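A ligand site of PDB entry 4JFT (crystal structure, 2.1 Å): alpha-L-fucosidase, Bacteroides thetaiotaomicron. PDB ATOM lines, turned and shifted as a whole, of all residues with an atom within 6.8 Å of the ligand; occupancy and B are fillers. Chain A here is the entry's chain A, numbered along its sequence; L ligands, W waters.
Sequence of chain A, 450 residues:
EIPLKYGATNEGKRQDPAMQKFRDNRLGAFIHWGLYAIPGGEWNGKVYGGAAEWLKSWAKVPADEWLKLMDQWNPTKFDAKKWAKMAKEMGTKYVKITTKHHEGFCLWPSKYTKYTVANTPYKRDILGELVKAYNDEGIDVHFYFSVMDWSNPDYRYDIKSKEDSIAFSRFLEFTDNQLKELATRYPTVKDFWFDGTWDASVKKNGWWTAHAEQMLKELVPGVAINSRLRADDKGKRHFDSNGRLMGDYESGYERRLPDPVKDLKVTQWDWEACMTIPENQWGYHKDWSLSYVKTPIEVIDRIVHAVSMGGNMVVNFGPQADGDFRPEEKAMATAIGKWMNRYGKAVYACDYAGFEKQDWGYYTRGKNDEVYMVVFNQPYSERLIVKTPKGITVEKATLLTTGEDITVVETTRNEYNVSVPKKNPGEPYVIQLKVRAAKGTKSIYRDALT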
ATOM      1  N   PHE A  30      -0.152  -4.964  10.762  1.00  0.00           N
ATOM      2  CA  PHE A  30       0.934  -4.143  11.361  1.00  0.00           C
ATOM      3  C   PHE A  30       0.997  -2.886  10.515  1.00  0.00           C
ATOM      4  O   PHE A  30       0.797  -2.928   9.294  1.00  0.00           O
ATOM      5  CB  PHE A  30       2.260  -4.872  11.264  1.00  0.00           C
ATOM      6  CG  PHE A  30       3.116  -4.789  12.490  1.00  0.00           C
ATOM      7  CD1 PHE A  30       3.491  -3.587  13.013  1.00  0.00           C
ATOM      8  CD2 PHE A  30       3.569  -5.944  13.099  1.00  0.00           C
ATOM      9  CE1 PHE A  30       4.305  -3.509  14.116  1.00  0.00           C
ATOM     10  CE2 PHE A  30       4.376  -5.894  14.236  1.00  0.00           C
ATOM     11  CZ  PHE A  30       4.748  -4.661  14.738  1.00  0.00           C
ATOM     12  N   HIS A  32       3.792   0.027   9.796  1.00  0.00           N
ATOM     13  CA  HIS A  32       5.089   0.703   9.937  1.00  0.00           C
ATOM     14  C   HIS A  32       5.025   2.047   9.194  1.00  0.00           C
ATOM     15  O   HIS A  32       4.910   2.097   7.977  1.00  0.00           O
ATOM     16  CB  HIS A  32       6.250  -0.099   9.371  1.00  0.00           C
ATOM     17  CG  HIS A  32       6.807  -1.097  10.319  1.00  0.00           C
ATOM     18  ND1 HIS A  32       6.122  -2.260  10.638  1.00  0.00           N
ATOM     19  CD2 HIS A  32       7.965  -1.138  10.999  1.00  0.00           C
ATOM     20  CE1 HIS A  32       6.841  -2.945  11.525  1.00  0.00           C
ATOM     21  NE2 HIS A  32       7.963  -2.291  11.751  1.00  0.00           N
ATOM     22  N   ALA A  51      15.990  -2.941   4.117  1.00  0.00           N
ATOM     23  CA  ALA A  51      14.708  -2.480   4.628  1.00  0.00           C
ATOM     24  C   ALA A  51      14.632  -0.918   4.706  1.00  0.00           C
ATOM     25  O   ALA A  51      15.503  -0.231   5.227  1.00  0.00           O
ATOM     26  CB  ALA A  51      14.474  -3.114   5.979  1.00  0.00           C
ATOM     27  N   GLU A  53      12.937   1.167   6.402  1.00  0.00           N
ATOM     28  CA  GLU A  53      12.919   1.804   7.716  1.00  0.00           C
ATOM     29  C   GLU A  53      14.313   1.907   8.387  1.00  0.00           C
ATOM     30  O   GLU A  53      14.498   2.617   9.390  1.00  0.00           O
ATOM     31  CB  GLU A  53      11.837   1.142   8.609  1.00  0.00           C
ATOM     32  CG  GLU A  53      12.139  -0.272   9.133  1.00  0.00           C
ATOM     33  CD  GLU A  53      12.012  -1.393   8.130  1.00  0.00           C
ATOM     34  OE1 GLU A  53      11.490  -1.212   7.027  1.00  0.00           O
ATOM     35  OE2 GLU A  53      12.386  -2.503   8.501  1.00  0.00           O
ATOM     36  N   TRP A  54      15.287   1.194   7.850  1.00  0.00           N
ATOM     37  CA  TRP A  54      16.696   1.278   8.261  1.00  0.00           C
ATOM     38  C   TRP A  54      17.519   2.106   7.246  1.00  0.00           C
ATOM     39  O   TRP A  54      18.724   2.019   7.204  1.00  0.00           O
ATOM     40  CB  TRP A  54      17.338  -0.130   8.334  1.00  0.00           C
ATOM     41  CG  TRP A  54      17.036  -0.880   9.538  1.00  0.00           C
ATOM     42  CD1 TRP A  54      15.836  -1.467   9.886  1.00  0.00           C
ATOM     43  CD2 TRP A  54      17.953  -1.172  10.602  1.00  0.00           C
ATOM     44  NE1 TRP A  54      15.969  -2.085  11.119  1.00  0.00           N
ATOM     45  CE2 TRP A  54      17.244  -1.911  11.571  1.00  0.00           C
ATOM     46  CE3 TRP A  54      19.298  -0.858  10.829  1.00  0.00           C
ATOM     47  CZ2 TRP A  54      17.848  -2.344  12.738  1.00  0.00           C
ATOM     48  CZ3 TRP A  54      19.900  -1.295  11.951  1.00  0.00           C
ATOM     49  CH2 TRP A  54      19.179  -2.034  12.912  1.00  0.00           C
ATOM     50  N   THR A  98       3.575   1.229  14.761  1.00  0.00           N
ATOM     51  CA  THR A  98       4.863   1.791  15.188  1.00  0.00           C
ATOM     52  C   THR A  98       4.583   3.192  15.806  1.00  0.00           C
ATOM     53  O   THR A  98       4.305   4.149  15.098  1.00  0.00           O
ATOM     54  CB  THR A  98       5.767   2.030  13.994  1.00  0.00           C
ATOM     55  OG1 THR A  98       5.006   2.721  13.010  1.00  0.00           O
ATOM     56  CG2 THR A  98       6.298   0.750  13.432  1.00  0.00           C
ATOM     57  N   HIS A 101       9.818   4.155  15.855  1.00  0.00           N
ATOM     58  CA  HIS A 101      10.764   3.164  15.363  1.00  0.00           C
ATOM     59  C   HIS A 101      12.182   3.615  15.744  1.00  0.00           C
ATOM     60  O   HIS A 101      12.356   4.555  16.573  1.00  0.00           O
ATOM     61  CB  HIS A 101      10.599   2.975  13.852  1.00  0.00           C
ATOM     62  CG  HIS A 101      11.030   1.632  13.364  1.00  0.00           C
ATOM     63  ND1 HIS A 101      12.279   1.388  12.852  1.00  0.00           N
ATOM     64  CD2 HIS A 101      10.373   0.451  13.323  1.00  0.00           C
ATOM     65  CE1 HIS A 101      12.384   0.114  12.547  1.00  0.00           C
ATOM     66  NE2 HIS A 101      11.243  -0.477  12.816  1.00  0.00           N
ATOM     67  N   HIS A 102      13.193   2.900  15.264  1.00  0.00           N
ATOM     68  CA  HIS A 102      14.607   3.171  15.743  1.00  0.00           C
ATOM     69  C   HIS A 102      15.004   4.633  15.497  1.00  0.00           C
ATOM     70  O   HIS A 102      15.784   5.182  16.247  1.00  0.00           O
ATOM     71  CB  HIS A 102      15.652   2.283  15.083  1.00  0.00           C
ATOM     72  CG  HIS A 102      15.276   0.827  14.989  1.00  0.00           C
ATOM     73  ND1 HIS A 102      14.666   0.151  16.013  1.00  0.00           N
ATOM     74  CD2 HIS A 102      15.420  -0.065  13.989  1.00  0.00           C
ATOM     75  CE1 HIS A 102      14.473  -1.102  15.661  1.00  0.00           C
ATOM     76  NE2 HIS A 102      14.929  -1.260  14.439  1.00  0.00           N
ATOM     77  N   TYR A 144       3.670  -0.953  18.798  1.00  0.00           N
ATOM     78  CA  TYR A 144       5.063  -1.223  18.605  1.00  0.00           C
ATOM     79  C   TYR A 144       5.823  -0.041  19.211  1.00  0.00           C
ATOM     80  O   TYR A 144       5.469   1.103  18.957  1.00  0.00           O
ATOM     81  CB  TYR A 144       5.337  -1.328  17.105  1.00  0.00           C
ATOM     82  CG  TYR A 144       6.798  -1.343  16.763  1.00  0.00           C
ATOM     83  CD1 TYR A 144       7.593  -0.197  16.902  1.00  0.00           C
ATOM     84  CD2 TYR A 144       7.409  -2.484  16.223  1.00  0.00           C
ATOM     85  CE1 TYR A 144       8.941  -0.188  16.582  1.00  0.00           C
ATOM     86  CE2 TYR A 144       8.775  -2.485  15.939  1.00  0.00           C
ATOM     87  CZ  TYR A 144       9.520  -1.341  16.099  1.00  0.00           C
ATOM     88  OH  TYR A 144      10.855  -1.343  15.821  1.00  0.00           O
ATOM     89  N   MET A 148      15.674   0.962  21.288  1.00  0.00           N
ATOM     90  CA  MET A 148      16.789   1.565  20.529  1.00  0.00           C
ATOM     91  C   MET A 148      16.296   2.826  19.881  1.00  0.00           C
ATOM     92  O   MET A 148      15.206   2.839  19.262  1.00  0.00           O
ATOM     93  CB  MET A 148      17.353   0.604  19.436  1.00  0.00           C
ATOM     94  CG  MET A 148      18.530   1.148  18.674  1.00  0.00           C
ATOM     95  SD  MET A 148      19.446   0.018  17.541  1.00  0.00           S
ATOM     96  CE  MET A 148      18.203  -0.455  16.418  1.00  0.00           C
ATOM     97  N   TRP A 193       4.483  -4.098  22.034  1.00  0.00           N
ATOM     98  CA  TRP A 193       5.332  -4.965  21.293  1.00  0.00           C
ATOM     99  C   TRP A 193       6.663  -4.260  21.210  1.00  0.00           C
ATOM    100  O   TRP A 193       6.839  -3.344  20.421  1.00  0.00           O
ATOM    101  CB  TRP A 193       4.736  -5.163  19.915  1.00  0.00           C
ATOM    102  CG  TRP A 193       5.251  -6.365  19.135  1.00  0.00           C
ATOM    103  CD1 TRP A 193       4.723  -7.629  19.144  1.00  0.00           C
ATOM    104  CD2 TRP A 193       6.371  -6.426  18.240  1.00  0.00           C
ATOM    105  NE1 TRP A 193       5.426  -8.466  18.305  1.00  0.00           N
ATOM    106  CE2 TRP A 193       6.449  -7.762  17.744  1.00  0.00           C
ATOM    107  CE3 TRP A 193       7.300  -5.482  17.788  1.00  0.00           C
ATOM    108  CZ2 TRP A 193       7.388  -8.169  16.816  1.00  0.00           C
ATOM    109  CZ3 TRP A 193       8.286  -5.895  16.880  1.00  0.00           C
ATOM    110  CH2 TRP A 193       8.320  -7.226  16.396  1.00  0.00           C
ATOM    111  N   ASP A 195      10.643  -3.644  20.359  1.00  0.00           N
ATOM    112  CA  ASP A 195      11.702  -3.973  19.412  1.00  0.00           C
ATOM    113  C   ASP A 195      12.956  -3.247  19.853  1.00  0.00           C
ATOM    114  O   ASP A 195      12.898  -2.416  20.768  1.00  0.00           O
ATOM    115  CB  ASP A 195      11.291  -3.512  18.029  1.00  0.00           C
ATOM    116  CG  ASP A 195      11.953  -4.276  16.889  1.00  0.00           C
ATOM    117  OD1 ASP A 195      12.717  -5.237  17.089  1.00  0.00           O
ATOM    118  OD2 ASP A 195      11.694  -3.852  15.752  1.00  0.00           O
ATOM    119  N   GLY A 196      14.080  -3.564  19.212  1.00  0.00           N
ATOM    120  CA  GLY A 196      15.366  -2.937  19.512  1.00  0.00           C
ATOM    121  C   GLY A 196      15.781  -3.060  20.953  1.00  0.00           C
ATOM    122  O   GLY A 196      16.180  -2.078  21.607  1.00  0.00           O
ATOM    123  N   TRP A 198      17.935  -5.885  21.658  1.00  0.00           N
ATOM    124  CA  TRP A 198      19.011  -6.880  21.528  1.00  0.00           C
ATOM    125  C   TRP A 198      20.431  -6.355  21.870  1.00  0.00           C
ATOM    126  O   TRP A 198      21.330  -7.141  21.997  1.00  0.00           O
ATOM    127  CB  TRP A 198      19.036  -7.476  20.098  1.00  0.00           C
ATOM    128  CG  TRP A 198      19.149  -6.437  19.085  1.00  0.00           C
ATOM    129  CD1 TRP A 198      20.254  -5.690  18.772  1.00  0.00           C
ATOM    130  CD2 TRP A 198      18.082  -5.948  18.299  1.00  0.00           C
ATOM    131  NE1 TRP A 198      19.930  -4.776  17.841  1.00  0.00           N
ATOM    132  CE2 TRP A 198      18.599  -4.905  17.538  1.00  0.00           C
ATOM    133  CE3 TRP A 198      16.732  -6.315  18.163  1.00  0.00           C
ATOM    134  CZ2 TRP A 198      17.798  -4.204  16.631  1.00  0.00           C
ATOM    135  CZ3 TRP A 198      15.953  -5.642  17.285  1.00  0.00           C
ATOM    136  CH2 TRP A 198      16.479  -4.595  16.522  1.00  0.00           C
ATOM    137  N   ARG A 228       9.946 -10.274  23.176  1.00  0.00           N
ATOM    138  CA  ARG A 228      11.161  -9.644  22.688  1.00  0.00           C
ATOM    139  C   ARG A 228      11.618  -8.483  23.623  1.00  0.00           C
ATOM    140  O   ARG A 228      12.800  -8.090  23.632  1.00  0.00           O
ATOM    141  CB  ARG A 228      10.906  -9.178  21.273  1.00  0.00           C
ATOM    142  CG  ARG A 228      12.024  -8.445  20.583  1.00  0.00           C
ATOM    143  CD  ARG A 228      11.642  -8.105  19.160  1.00  0.00           C
ATOM    144  NE  ARG A 228      12.014  -9.242  18.336  1.00  0.00           N
ATOM    145  CZ  ARG A 228      11.212  -9.927  17.519  1.00  0.00           C
ATOM    146  NH1 ARG A 228       9.950  -9.611  17.332  1.00  0.00           N
ATOM    147  NH2 ARG A 228      11.699 -10.954  16.864  1.00  0.00           N
ATOM    148  N   GLU A 254       9.098 -14.241  12.232  1.00  0.00           N
ATOM    149  CA  GLU A 254       9.168 -13.245  11.158  1.00  0.00           C
ATOM    150  C   GLU A 254       9.666 -13.835   9.813  1.00  0.00           C
ATOM    151  O   GLU A 254       8.977 -13.695   8.817  1.00  0.00           O
ATOM    152  CB  GLU A 254       9.958 -12.002  11.617  1.00  0.00           C
ATOM    153  CG  GLU A 254      10.234 -12.040  13.130  1.00  0.00           C
ATOM    154  CD  GLU A 254       9.855 -10.805  13.904  1.00  0.00           C
ATOM    155  OE1 GLU A 254      10.420  -9.685  13.628  1.00  0.00           O
ATOM    156  OE2 GLU A 254       8.990 -10.984  14.829  1.00  0.00           O
ATOM    157  N   CYS A 274       4.698 -12.085  12.788  1.00  0.00           N
ATOM    158  CA  CYS A 274       4.469 -10.888  12.005  1.00  0.00           C
ATOM    159  C   CYS A 274       5.227 -11.089  10.680  1.00  0.00           C
ATOM    160  O   CYS A 274       6.342 -11.574  10.707  1.00  0.00           O
ATOM    161  CB  CYS A 274       5.013  -9.712  12.786  1.00  0.00           C
ATOM    162  SG  CYS A 274       4.100  -9.345  14.324  1.00  0.00           S
ATOM    163  N   ASN A 280      11.631  -8.483   2.820  1.00  0.00           N
ATOM    164  CA  ASN A 280      12.064  -7.801   4.009  1.00  0.00           C
ATOM    165  C   ASN A 280      11.934  -6.246   3.933  1.00  0.00           C
ATOM    166  O   ASN A 280      12.917  -5.539   4.121  1.00  0.00           O
ATOM    167  CB  ASN A 280      13.507  -8.171   4.344  1.00  0.00           C
ATOM    168  CG  ASN A 280      13.897  -7.713   5.732  1.00  0.00           C
ATOM    169  OD1 ASN A 280      13.055  -7.285   6.527  1.00  0.00           O
ATOM    170  ND2 ASN A 280      15.185  -7.798   6.031  1.00  0.00           N
ATOM    171  N   TRP A 282       9.436  -3.418   5.803  1.00  0.00           N
ATOM    172  CA  TRP A 282       8.358  -3.096   6.752  1.00  0.00           C
ATOM    173  C   TRP A 282       7.856  -1.680   6.499  1.00  0.00           C
ATOM    174  O   TRP A 282       6.665  -1.447   6.189  1.00  0.00           O
ATOM    175  CB  TRP A 282       8.873  -3.209   8.164  1.00  0.00           C
ATOM    176  CG  TRP A 282       9.342  -4.567   8.521  1.00  0.00           C
ATOM    177  CD1 TRP A 282      10.575  -5.079   8.328  1.00  0.00           C
ATOM    178  CD2 TRP A 282       8.569  -5.604   9.166  1.00  0.00           C
ATOM    179  NE1 TRP A 282      10.633  -6.326   8.793  1.00  0.00           N
ATOM    180  CE2 TRP A 282       9.438  -6.687   9.353  1.00  0.00           C
ATOM    181  CE3 TRP A 282       7.263  -5.697   9.631  1.00  0.00           C
ATOM    182  CZ2 TRP A 282       9.028  -7.893   9.966  1.00  0.00           C
ATOM    183  CZ3 TRP A 282       6.840  -6.900  10.227  1.00  0.00           C
ATOM    184  CH2 TRP A 282       7.726  -7.984  10.377  1.00  0.00           C
ATOM    185  N   GLY A 283       8.762  -0.719   6.569  1.00  0.00           N
ATOM    186  CA  GLY A 283       8.410   0.638   6.088  1.00  0.00           C
ATOM    187  C   GLY A 283       8.200   0.672   4.581  1.00  0.00           C
ATOM    188  O   GLY A 283       8.662  -0.215   3.819  1.00  0.00           O
HETATM  189  C1  LIG L   1      17.916  -8.635  11.862  1.00  0.00           C
HETATM  190  O1  LIG L   1      17.806  -7.290  12.390  1.00  0.00           O
HETATM  191  C2  LIG L   1      16.568  -6.670  12.460  1.00  0.00           C
HETATM  192  C3  LIG L   1      15.463  -7.097  11.749  1.00  0.00           C
HETATM  193  C4  LIG L   1      14.256  -6.403  11.851  1.00  0.00           C
HETATM  194  C5  LIG L   1      16.465  -5.528  13.227  1.00  0.00           C
HETATM  195  C6  LIG L   1      15.281  -4.839  13.333  1.00  0.00           C
HETATM  196  C7  LIG L   1      14.156  -5.262  12.650  1.00  0.00           C
HETATM  197  C8  LIG L   1      12.928  -4.556  12.815  1.00  0.00           C
HETATM  198  N1  LIG L   1      11.899  -5.499  13.452  1.00  0.00           N
HETATM  199  C9  LIG L   1      10.776  -5.508  12.496  1.00  0.00           C
HETATM  200  C10 LIG L   1       9.439  -5.912  13.082  1.00  0.00           C
HETATM  201  C11 LIG L   1      10.774  -4.014  11.946  1.00  0.00           C
HETATM  202  O2  LIG L   1      10.405  -3.080  12.977  1.00  0.00           O
HETATM  203  C12 LIG L   1      12.293  -4.061  11.536  1.00  0.00           C
HETATM  204  O3  LIG L   1      12.864  -2.832  11.037  1.00  0.00           O
HETATM  205  O   HOH W   1      12.824  -7.771  15.853  1.00  0.00           O
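OD2 of Asp 195 lies within salt-bridge range of N1 of the ligand (2.8 Å). A ring nitrogen (NE2) of His 101 lies within hydrogen-bond range of an oxygen (O2) of the ligand (2.7 Å). O3 of the ligand is in hydrogen-bond range of OE2 of Glu 53 (2.6 Å). An oxygen (O2) of the ligand lies within hydrogen-bond range of the side-chain hydroxyl (OH) of Tyr 144 (3.4 Å). An oxygen (O2) of the ligand sits at hydrogen-bond distance from a ring nitrogen (NE2) of His 32 (2.8 Å). The indole nitrogen (NE1) of Trp 54 sits at hydrogen-bond distance from an oxygen (O3) of the ligand (3.2 Å).
The side-chain amide oxygen of Asn 280 lies within hydrogen-bond range of the indole nitrogen of Trp 282 (3.5 Å). The backbone NH (N) of Trp 282 is in hydrogen-bond range of the side-chain carboxylate (OE1) of Glu 53 (3.3 Å). OE1 of Glu 53 is in hydrogen-bond range of N of Gly 283 (2.8 Å). The side-chain carboxylate (OD2) of Asp 195 sits at hydrogen-bond distance from the side-chain hydroxyl (OH) of Tyr 144 (2.6 Å). NE2 of His 101 sits close to OH of Tyr 144, 3.2 Å away. The side-chain carboxylate (OE2) of Glu 254 is in salt-bridge range of the guanidinium group (NH1) of Arg 228, 3.0 Å away.
Residues that only touch the ligand: His 102, Trp 193, Trp 198, Glu 254 and Trp 282. Hydrophobic or aromatic side chains within 4 Å of the ligand: His 32, Trp 54, His 101, Tyr 144, Trp 193, Trp 198 and Trp 282. Within 4 Å of the ligand: His 32, Glu 53, Trp 54, His 101, His 102, Tyr 144, Trp 193, Asp 195, Trp 198, Glu 254 and Trp 282.
Water W1 lies within hydrogen-bond range of OD1 of Asp 195 (2.8 Å), NE of Arg 228 (3.0 Å) and N1 of the ligand (3.4 Å).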
